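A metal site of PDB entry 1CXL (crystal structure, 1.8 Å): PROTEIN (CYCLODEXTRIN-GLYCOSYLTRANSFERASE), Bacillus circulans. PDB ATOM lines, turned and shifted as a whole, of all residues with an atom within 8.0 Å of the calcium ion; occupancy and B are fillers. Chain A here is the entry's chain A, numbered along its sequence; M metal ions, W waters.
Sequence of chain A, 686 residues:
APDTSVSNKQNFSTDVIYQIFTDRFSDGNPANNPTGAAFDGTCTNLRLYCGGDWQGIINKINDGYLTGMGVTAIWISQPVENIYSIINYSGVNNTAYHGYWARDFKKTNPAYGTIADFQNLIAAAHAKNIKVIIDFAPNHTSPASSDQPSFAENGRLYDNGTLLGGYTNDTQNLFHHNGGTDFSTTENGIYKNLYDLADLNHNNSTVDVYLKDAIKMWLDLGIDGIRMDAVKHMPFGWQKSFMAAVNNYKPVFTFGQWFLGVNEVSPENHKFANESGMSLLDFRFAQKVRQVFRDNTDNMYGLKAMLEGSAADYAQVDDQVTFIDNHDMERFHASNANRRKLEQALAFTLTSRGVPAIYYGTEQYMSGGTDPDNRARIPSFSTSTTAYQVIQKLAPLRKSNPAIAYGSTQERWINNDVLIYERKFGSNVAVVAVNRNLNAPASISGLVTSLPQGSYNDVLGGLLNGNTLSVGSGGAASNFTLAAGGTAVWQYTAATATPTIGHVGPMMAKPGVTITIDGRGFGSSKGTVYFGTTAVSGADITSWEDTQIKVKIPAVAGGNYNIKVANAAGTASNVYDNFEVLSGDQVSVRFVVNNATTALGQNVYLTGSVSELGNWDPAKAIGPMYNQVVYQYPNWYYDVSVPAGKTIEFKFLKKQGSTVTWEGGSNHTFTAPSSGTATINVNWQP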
ATOM      1  N   THR A  22     -30.370  15.760  29.440  1.00  0.00           N
ATOM      2  CA  THR A  22     -29.781  16.691  28.503  1.00  0.00           C
ATOM      3  C   THR A  22     -30.042  18.161  28.733  1.00  0.00           C
ATOM      4  O   THR A  22     -29.109  18.961  28.775  1.00  0.00           O
ATOM      5  CB  THR A  22     -30.036  16.281  27.058  1.00  0.00           C
ATOM      6  OG1 THR A  22     -29.597  14.949  26.893  1.00  0.00           O
ATOM      7  CG2 THR A  22     -29.261  17.197  26.110  1.00  0.00           C
ATOM      8  N   ASP A  23     -31.303  18.497  28.887  1.00  0.00           N
ATOM      9  CA  ASP A  23     -31.687  19.890  29.067  1.00  0.00           C
ATOM     10  C   ASP A  23     -31.159  20.520  30.346  1.00  0.00           C
ATOM     11  O   ASP A  23     -31.031  21.741  30.440  1.00  0.00           O
ATOM     12  CB  ASP A  23     -33.221  20.026  29.075  1.00  0.00           C
ATOM     13  CG  ASP A  23     -33.630  21.478  29.064  1.00  0.00           C
ATOM     14  OD1 ASP A  23     -33.287  22.246  28.171  1.00  0.00           O
ATOM     15  OD2 ASP A  23     -34.332  21.837  30.115  1.00  0.00           O
ATOM     16  N   SER A  26     -25.800  20.932  30.540  1.00  0.00           N
ATOM     17  CA  SER A  26     -25.002  22.055  30.106  1.00  0.00           C
ATOM     18  C   SER A  26     -25.476  22.613  28.770  1.00  0.00           C
ATOM     19  O   SER A  26     -25.574  21.890  27.781  1.00  0.00           O
ATOM     20  CB  SER A  26     -23.535  21.672  30.013  1.00  0.00           C
ATOM     21  OG  SER A  26     -22.753  22.801  29.627  1.00  0.00           O
ATOM     22  N   ASP A  27     -25.783  23.907  28.754  1.00  0.00           N
ATOM     23  CA  ASP A  27     -26.209  24.570  27.515  1.00  0.00           C
ATOM     24  C   ASP A  27     -24.964  25.034  26.785  1.00  0.00           C
ATOM     25  O   ASP A  27     -24.434  26.107  27.082  1.00  0.00           O
ATOM     26  CB  ASP A  27     -27.158  25.754  27.799  1.00  0.00           C
ATOM     27  CG  ASP A  27     -27.545  26.549  26.579  1.00  0.00           C
ATOM     28  OD1 ASP A  27     -27.334  26.170  25.446  1.00  0.00           O
ATOM     29  OD2 ASP A  27     -28.147  27.673  26.859  1.00  0.00           O
ATOM     30  N   GLY A  28     -24.456  24.209  25.864  1.00  0.00           N
ATOM     31  CA  GLY A  28     -23.243  24.554  25.134  1.00  0.00           C
ATOM     32  C   GLY A  28     -23.512  25.388  23.889  1.00  0.00           C
ATOM     33  O   GLY A  28     -22.589  25.921  23.278  1.00  0.00           O
ATOM     34  N   ASN A  29     -24.767  25.500  23.500  1.00  0.00           N
ATOM     35  CA  ASN A  29     -25.128  26.268  22.340  1.00  0.00           C
ATOM     36  C   ASN A  29     -26.428  26.976  22.574  1.00  0.00           C
ATOM     37  O   ASN A  29     -27.495  26.415  22.381  1.00  0.00           O
ATOM     38  CB  ASN A  29     -25.242  25.359  21.105  1.00  0.00           C
ATOM     39  CG  ASN A  29     -25.678  26.127  19.882  1.00  0.00           C
ATOM     40  OD1 ASN A  29     -25.723  27.366  19.889  1.00  0.00           O
ATOM     41  ND2 ASN A  29     -25.988  25.405  18.813  1.00  0.00           N
ATOM     42  N   PRO A  30     -26.350  28.205  23.023  1.00  0.00           N
ATOM     43  CA  PRO A  30     -27.530  28.964  23.326  1.00  0.00           C
ATOM     44  C   PRO A  30     -28.359  29.264  22.114  1.00  0.00           C
ATOM     45  O   PRO A  30     -29.528  29.589  22.221  1.00  0.00           O
ATOM     46  CB  PRO A  30     -27.080  30.246  23.999  1.00  0.00           C
ATOM     47  CG  PRO A  30     -25.564  30.205  24.085  1.00  0.00           C
ATOM     48  CD  PRO A  30     -25.109  28.940  23.378  1.00  0.00           C
ATOM     49  N   ALA A  31     -27.737  29.145  20.947  1.00  0.00           N
ATOM     50  CA  ALA A  31     -28.438  29.436  19.707  1.00  0.00           C
ATOM     51  C   ALA A  31     -29.557  28.458  19.382  1.00  0.00           C
ATOM     52  O   ALA A  31     -30.456  28.774  18.615  1.00  0.00           O
ATOM     53  CB  ALA A  31     -27.460  29.596  18.552  1.00  0.00           C
ATOM     54  N   ASN A  32     -29.515  27.248  19.975  1.00  0.00           N
ATOM     55  CA  ASN A  32     -30.559  26.270  19.713  1.00  0.00           C
ATOM     56  C   ASN A  32     -31.603  26.241  20.817  1.00  0.00           C
ATOM     57  O   ASN A  32     -32.476  25.379  20.834  1.00  0.00           O
ATOM     58  CB  ASN A  32     -30.022  24.872  19.380  1.00  0.00           C
ATOM     59  CG  ASN A  32     -29.197  24.266  20.500  1.00  0.00           C
ATOM     60  OD1 ASN A  32     -29.383  24.623  21.669  1.00  0.00           O
ATOM     61  ND2 ASN A  32     -28.282  23.362  20.153  1.00  0.00           N
ATOM     62  N   ASN A  33     -31.515  27.170  21.743  1.00  0.00           N
ATOM     63  CA  ASN A  33     -32.457  27.222  22.835  1.00  0.00           C
ATOM     64  C   ASN A  33     -33.846  27.535  22.362  1.00  0.00           C
ATOM     65  O   ASN A  33     -34.043  28.425  21.532  1.00  0.00           O
ATOM     66  CB  ASN A  33     -32.074  28.291  23.869  1.00  0.00           C
ATOM     67  CG  ASN A  33     -30.778  27.994  24.584  1.00  0.00           C
ATOM     68  OD1 ASN A  33     -30.210  26.899  24.417  1.00  0.00           O
ATOM     69  ND2 ASN A  33     -30.306  28.949  25.376  1.00  0.00           N
ATOM     70  N   PRO A  34     -34.835  26.862  22.927  1.00  0.00           N
ATOM     71  CA  PRO A  34     -36.191  27.202  22.563  1.00  0.00           C
ATOM     72  C   PRO A  34     -36.442  28.614  23.056  1.00  0.00           C
ATOM     73  O   PRO A  34     -35.615  29.198  23.745  1.00  0.00           O
ATOM     74  CB  PRO A  34     -37.101  26.176  23.228  1.00  0.00           C
ATOM     75  CG  PRO A  34     -36.215  24.983  23.563  1.00  0.00           C
ATOM     76  CD  PRO A  34     -34.776  25.483  23.474  1.00  0.00           C
ATOM     77  N   PHE A  39     -39.317  28.472  27.219  1.00  0.00           N
ATOM     78  CA  PHE A  39     -37.985  28.553  27.748  1.00  0.00           C
ATOM     79  C   PHE A  39     -37.825  29.340  29.038  1.00  0.00           C
ATOM     80  O   PHE A  39     -38.555  30.287  29.300  1.00  0.00           O
ATOM     81  CB  PHE A  39     -37.122  29.183  26.651  1.00  0.00           C
ATOM     82  CG  PHE A  39     -35.653  29.237  26.964  1.00  0.00           C
ATOM     83  CD1 PHE A  39     -34.862  28.092  26.874  1.00  0.00           C
ATOM     84  CD2 PHE A  39     -35.051  30.434  27.336  1.00  0.00           C
ATOM     85  CE1 PHE A  39     -33.506  28.137  27.160  1.00  0.00           C
ATOM     86  CE2 PHE A  39     -33.691  30.500  27.627  1.00  0.00           C
ATOM     87  CZ  PHE A  39     -32.913  29.348  27.535  1.00  0.00           C
ATOM     88  N   TYR A  49     -37.982  24.364  28.976  1.00  0.00           N
ATOM     89  CA  TYR A  49     -36.634  24.045  28.534  1.00  0.00           C
ATOM     90  C   TYR A  49     -35.671  25.004  29.217  1.00  0.00           C
ATOM     91  O   TYR A  49     -35.968  26.201  29.346  1.00  0.00           O
ATOM     92  CB  TYR A  49     -36.465  24.205  27.007  1.00  0.00           C
ATOM     93  CG  TYR A  49     -36.853  23.011  26.167  1.00  0.00           C
ATOM     94  CD1 TYR A  49     -38.155  22.867  25.690  1.00  0.00           C
ATOM     95  CD2 TYR A  49     -35.905  22.054  25.782  1.00  0.00           C
ATOM     96  CE1 TYR A  49     -38.536  21.790  24.888  1.00  0.00           C
ATOM     97  CE2 TYR A  49     -36.266  20.968  24.978  1.00  0.00           C
ATOM     98  CZ  TYR A  49     -37.574  20.846  24.535  1.00  0.00           C
ATOM     99  OH  TYR A  49     -37.924  19.783  23.748  1.00  0.00           O
ATOM    100  N   CYS A  50     -34.509  24.495  29.630  1.00  0.00           N
ATOM    101  CA  CYS A  50     -33.502  25.320  30.273  1.00  0.00           C
ATOM    102  C   CYS A  50     -32.328  25.618  29.341  1.00  0.00           C
ATOM    103  O   CYS A  50     -31.531  26.537  29.578  1.00  0.00           O
ATOM    104  CB  CYS A  50     -33.044  24.775  31.633  1.00  0.00           C
ATOM    105  SG  CYS A  50     -34.421  24.594  32.786  1.00  0.00           S
ATOM    106  N   GLY A  51     -32.215  24.819  28.261  1.00  0.00           N
ATOM    107  CA  GLY A  51     -31.170  25.050  27.273  1.00  0.00           C
ATOM    108  C   GLY A  51     -30.063  23.994  27.162  1.00  0.00           C
ATOM    109  O   GLY A  51     -29.253  24.073  26.229  1.00  0.00           O
ATOM    110  N   GLY A  52     -29.997  23.047  28.096  1.00  0.00           N
ATOM    111  CA  GLY A  52     -28.952  22.020  28.057  1.00  0.00           C
ATOM    112  C   GLY A  52     -28.996  21.263  26.744  1.00  0.00           C
ATOM    113  O   GLY A  52     -30.073  20.911  26.280  1.00  0.00           O
ATOM    114  N   ASP A  53     -27.829  21.002  26.146  1.00  0.00           N
ATOM    115  CA  ASP A  53     -27.799  20.343  24.852  1.00  0.00           C
ATOM    116  C   ASP A  53     -26.579  19.456  24.615  1.00  0.00           C
ATOM    117  O   ASP A  53     -25.711  19.316  25.477  1.00  0.00           O
ATOM    118  CB  ASP A  53     -27.832  21.443  23.787  1.00  0.00           C
ATOM    119  CG  ASP A  53     -26.736  22.450  24.020  1.00  0.00           C
ATOM    120  OD1 ASP A  53     -25.649  22.150  24.461  1.00  0.00           O
ATOM    121  OD2 ASP A  53     -27.087  23.692  23.726  1.00  0.00           O
ATOM    122  N   TRP A  54     -26.493  18.887  23.415  1.00  0.00           N
ATOM    123  CA  TRP A  54     -25.389  18.005  23.079  1.00  0.00           C
ATOM    124  C   TRP A  54     -24.056  18.711  23.097  1.00  0.00           C
ATOM    125  O   TRP A  54     -23.039  18.143  23.503  1.00  0.00           O
ATOM    126  CB  TRP A  54     -25.598  17.156  21.819  1.00  0.00           C
ATOM    127  CG  TRP A  54     -26.806  16.291  21.911  1.00  0.00           C
ATOM    128  CD1 TRP A  54     -27.293  15.722  23.046  1.00  0.00           C
ATOM    129  CD2 TRP A  54     -27.689  15.896  20.848  1.00  0.00           C
ATOM    130  NE1 TRP A  54     -28.428  15.001  22.770  1.00  0.00           N
ATOM    131  CE2 TRP A  54     -28.708  15.098  21.437  1.00  0.00           C
ATOM    132  CE3 TRP A  54     -27.738  16.164  19.487  1.00  0.00           C
ATOM    133  CZ2 TRP A  54     -29.749  14.560  20.675  1.00  0.00           C
ATOM    134  CZ3 TRP A  54     -28.772  15.627  18.737  1.00  0.00           C
ATOM    135  CH2 TRP A  54     -29.758  14.828  19.325  1.00  0.00           C
ATOM    136  N   GLN A  55     -24.028  19.962  22.641  1.00  0.00           N
ATOM    137  CA  GLN A  55     -22.782  20.684  22.641  1.00  0.00           C
ATOM    138  C   GLN A  55     -22.259  20.796  24.065  1.00  0.00           C
ATOM    139  O   GLN A  55     -21.057  20.744  24.310  1.00  0.00           O
ATOM    140  CB  GLN A  55     -22.878  22.061  21.987  1.00  0.00           C
ATOM    141  CG  GLN A  55     -21.524  22.789  21.993  1.00  0.00           C
ATOM    142  CD  GLN A  55     -20.500  22.090  21.136  1.00  0.00           C
ATOM    143  OE1 GLN A  55     -20.740  21.824  19.939  1.00  0.00           O
ATOM    144  NE2 GLN A  55     -19.365  21.736  21.739  1.00  0.00           N
ATOM    145  N   GLY A  56     -23.193  20.934  24.988  1.00  0.00           N
ATOM    146  CA  GLY A  56     -22.862  21.044  26.393  1.00  0.00           C
ATOM    147  C   GLY A  56     -22.201  19.765  26.893  1.00  0.00           C
ATOM    148  O   GLY A  56     -21.195  19.797  27.591  1.00  0.00           O
ATOM    149  N   PRO A 110     -34.246  19.439  17.950  1.00  0.00           N
ATOM    150  CA  PRO A 110     -33.424  20.613  17.669  1.00  0.00           C
ATOM    151  C   PRO A 110     -32.896  21.327  18.887  1.00  0.00           C
ATOM    152  O   PRO A 110     -31.877  21.989  18.803  1.00  0.00           O
ATOM    153  CB  PRO A 110     -34.249  21.552  16.794  1.00  0.00           C
ATOM    154  CG  PRO A 110     -35.638  20.937  16.664  1.00  0.00           C
ATOM    155  CD  PRO A 110     -35.612  19.603  17.393  1.00  0.00           C
ATOM    156  N   ALA A 111     -33.589  21.212  20.017  1.00  0.00           N
ATOM    157  CA  ALA A 111     -33.109  21.865  21.231  1.00  0.00           C
ATOM    158  C   ALA A 111     -31.821  21.205  21.698  1.00  0.00           C
ATOM    159  O   ALA A 111     -30.922  21.858  22.240  1.00  0.00           O
ATOM    160  CB  ALA A 111     -34.168  21.850  22.326  1.00  0.00           C
ATOM    161  N   TYR A 112     -31.717  19.889  21.471  1.00  0.00           N
ATOM    162  CA  TYR A 112     -30.531  19.133  21.845  1.00  0.00           C
ATOM    163  C   TYR A 112     -29.431  19.345  20.814  1.00  0.00           C
ATOM    164  O   TYR A 112     -28.252  19.517  21.139  1.00  0.00           O
ATOM    165  CB  TYR A 112     -30.806  17.625  22.007  1.00  0.00           C
ATOM    166  CG  TYR A 112     -31.856  17.271  23.068  1.00  0.00           C
ATOM    167  CD1 TYR A 112     -32.240  18.168  24.063  1.00  0.00           C
ATOM    168  CD2 TYR A 112     -32.448  16.003  23.040  1.00  0.00           C
ATOM    169  CE1 TYR A 112     -33.189  17.808  25.023  1.00  0.00           C
ATOM    170  CE2 TYR A 112     -33.397  15.630  23.993  1.00  0.00           C
ATOM    171  CZ  TYR A 112     -33.769  16.534  24.989  1.00  0.00           C
ATOM    172  OH  TYR A 112     -34.720  16.167  25.917  1.00  0.00           O
ATOM    173  N   GLY A 113     -29.827  19.347  19.548  1.00  0.00           N
ATOM    174  CA  GLY A 113     -28.893  19.561  18.461  1.00  0.00           C
ATOM    175  C   GLY A 113     -29.371  18.980  17.145  1.00  0.00           C
ATOM    176  O   GLY A 113     -30.472  18.453  17.040  1.00  0.00           O
HETATM  177 CA    CA M   1     -28.865  25.135  24.035  1.00  0.00          CA
HETATM  178  O   HOH W   1     -31.060  23.986  23.980  1.00  0.00           O
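The nearest printed residue that does not touch the calcium ion is Pro 30 (4.1 Å).
The calcium ion is bound by OD1 of Asn 33 (2.3 Å).
The side-chain carboxylate (OD2) of Asp 53 binds the calcium ion, at 2.3 Å.
The calcium ion is bound by the side-chain carboxylate (OD1) of Asp 27 (2.3 Å).
The backbone carbonyl oxygen (O) of Gly 51 is bound to the calcium ion (2.5 Å).
The side-chain amide oxygen (OD1) of Asn 32 binds the calcium ion (2.5 Å).
Water W1 is bound to the calcium ion (2.5 Å).
O of Asn 29 is bound to the calcium ion, 2.5 Å away.
The backbone NH (N) of Gly 56 lies within hydrogen-bond range of the side-chain carboxylate (OD1) of Asp 53, at 2.8 Å.
N of Gln 55 lies close to OD1 of Asp 53.
The side-chain carboxylate of Asp 53 lies within hydrogen-bond range of the backbone NH of Gly 28.
The backbone carbonyl oxygen (O) of Pro 30 sits close to the side-chain amide nitrogen (ND2) of Asn 33 (3.3 Å).
N of Asp 53 lies within hydrogen-bond range of O of Ser 26.
OD1 of Asp 23 sits at hydrogen-bond distance from N of Gly 51, at 2.8 Å.
OD1 of Asn 29 sits at hydrogen-bond distance from N of Ala 31 (2.9 Å).
The side-chain amide oxygen of Asn 32 lies close to the backbone carbonyl oxygen of Ala 111 (3.2 Å).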
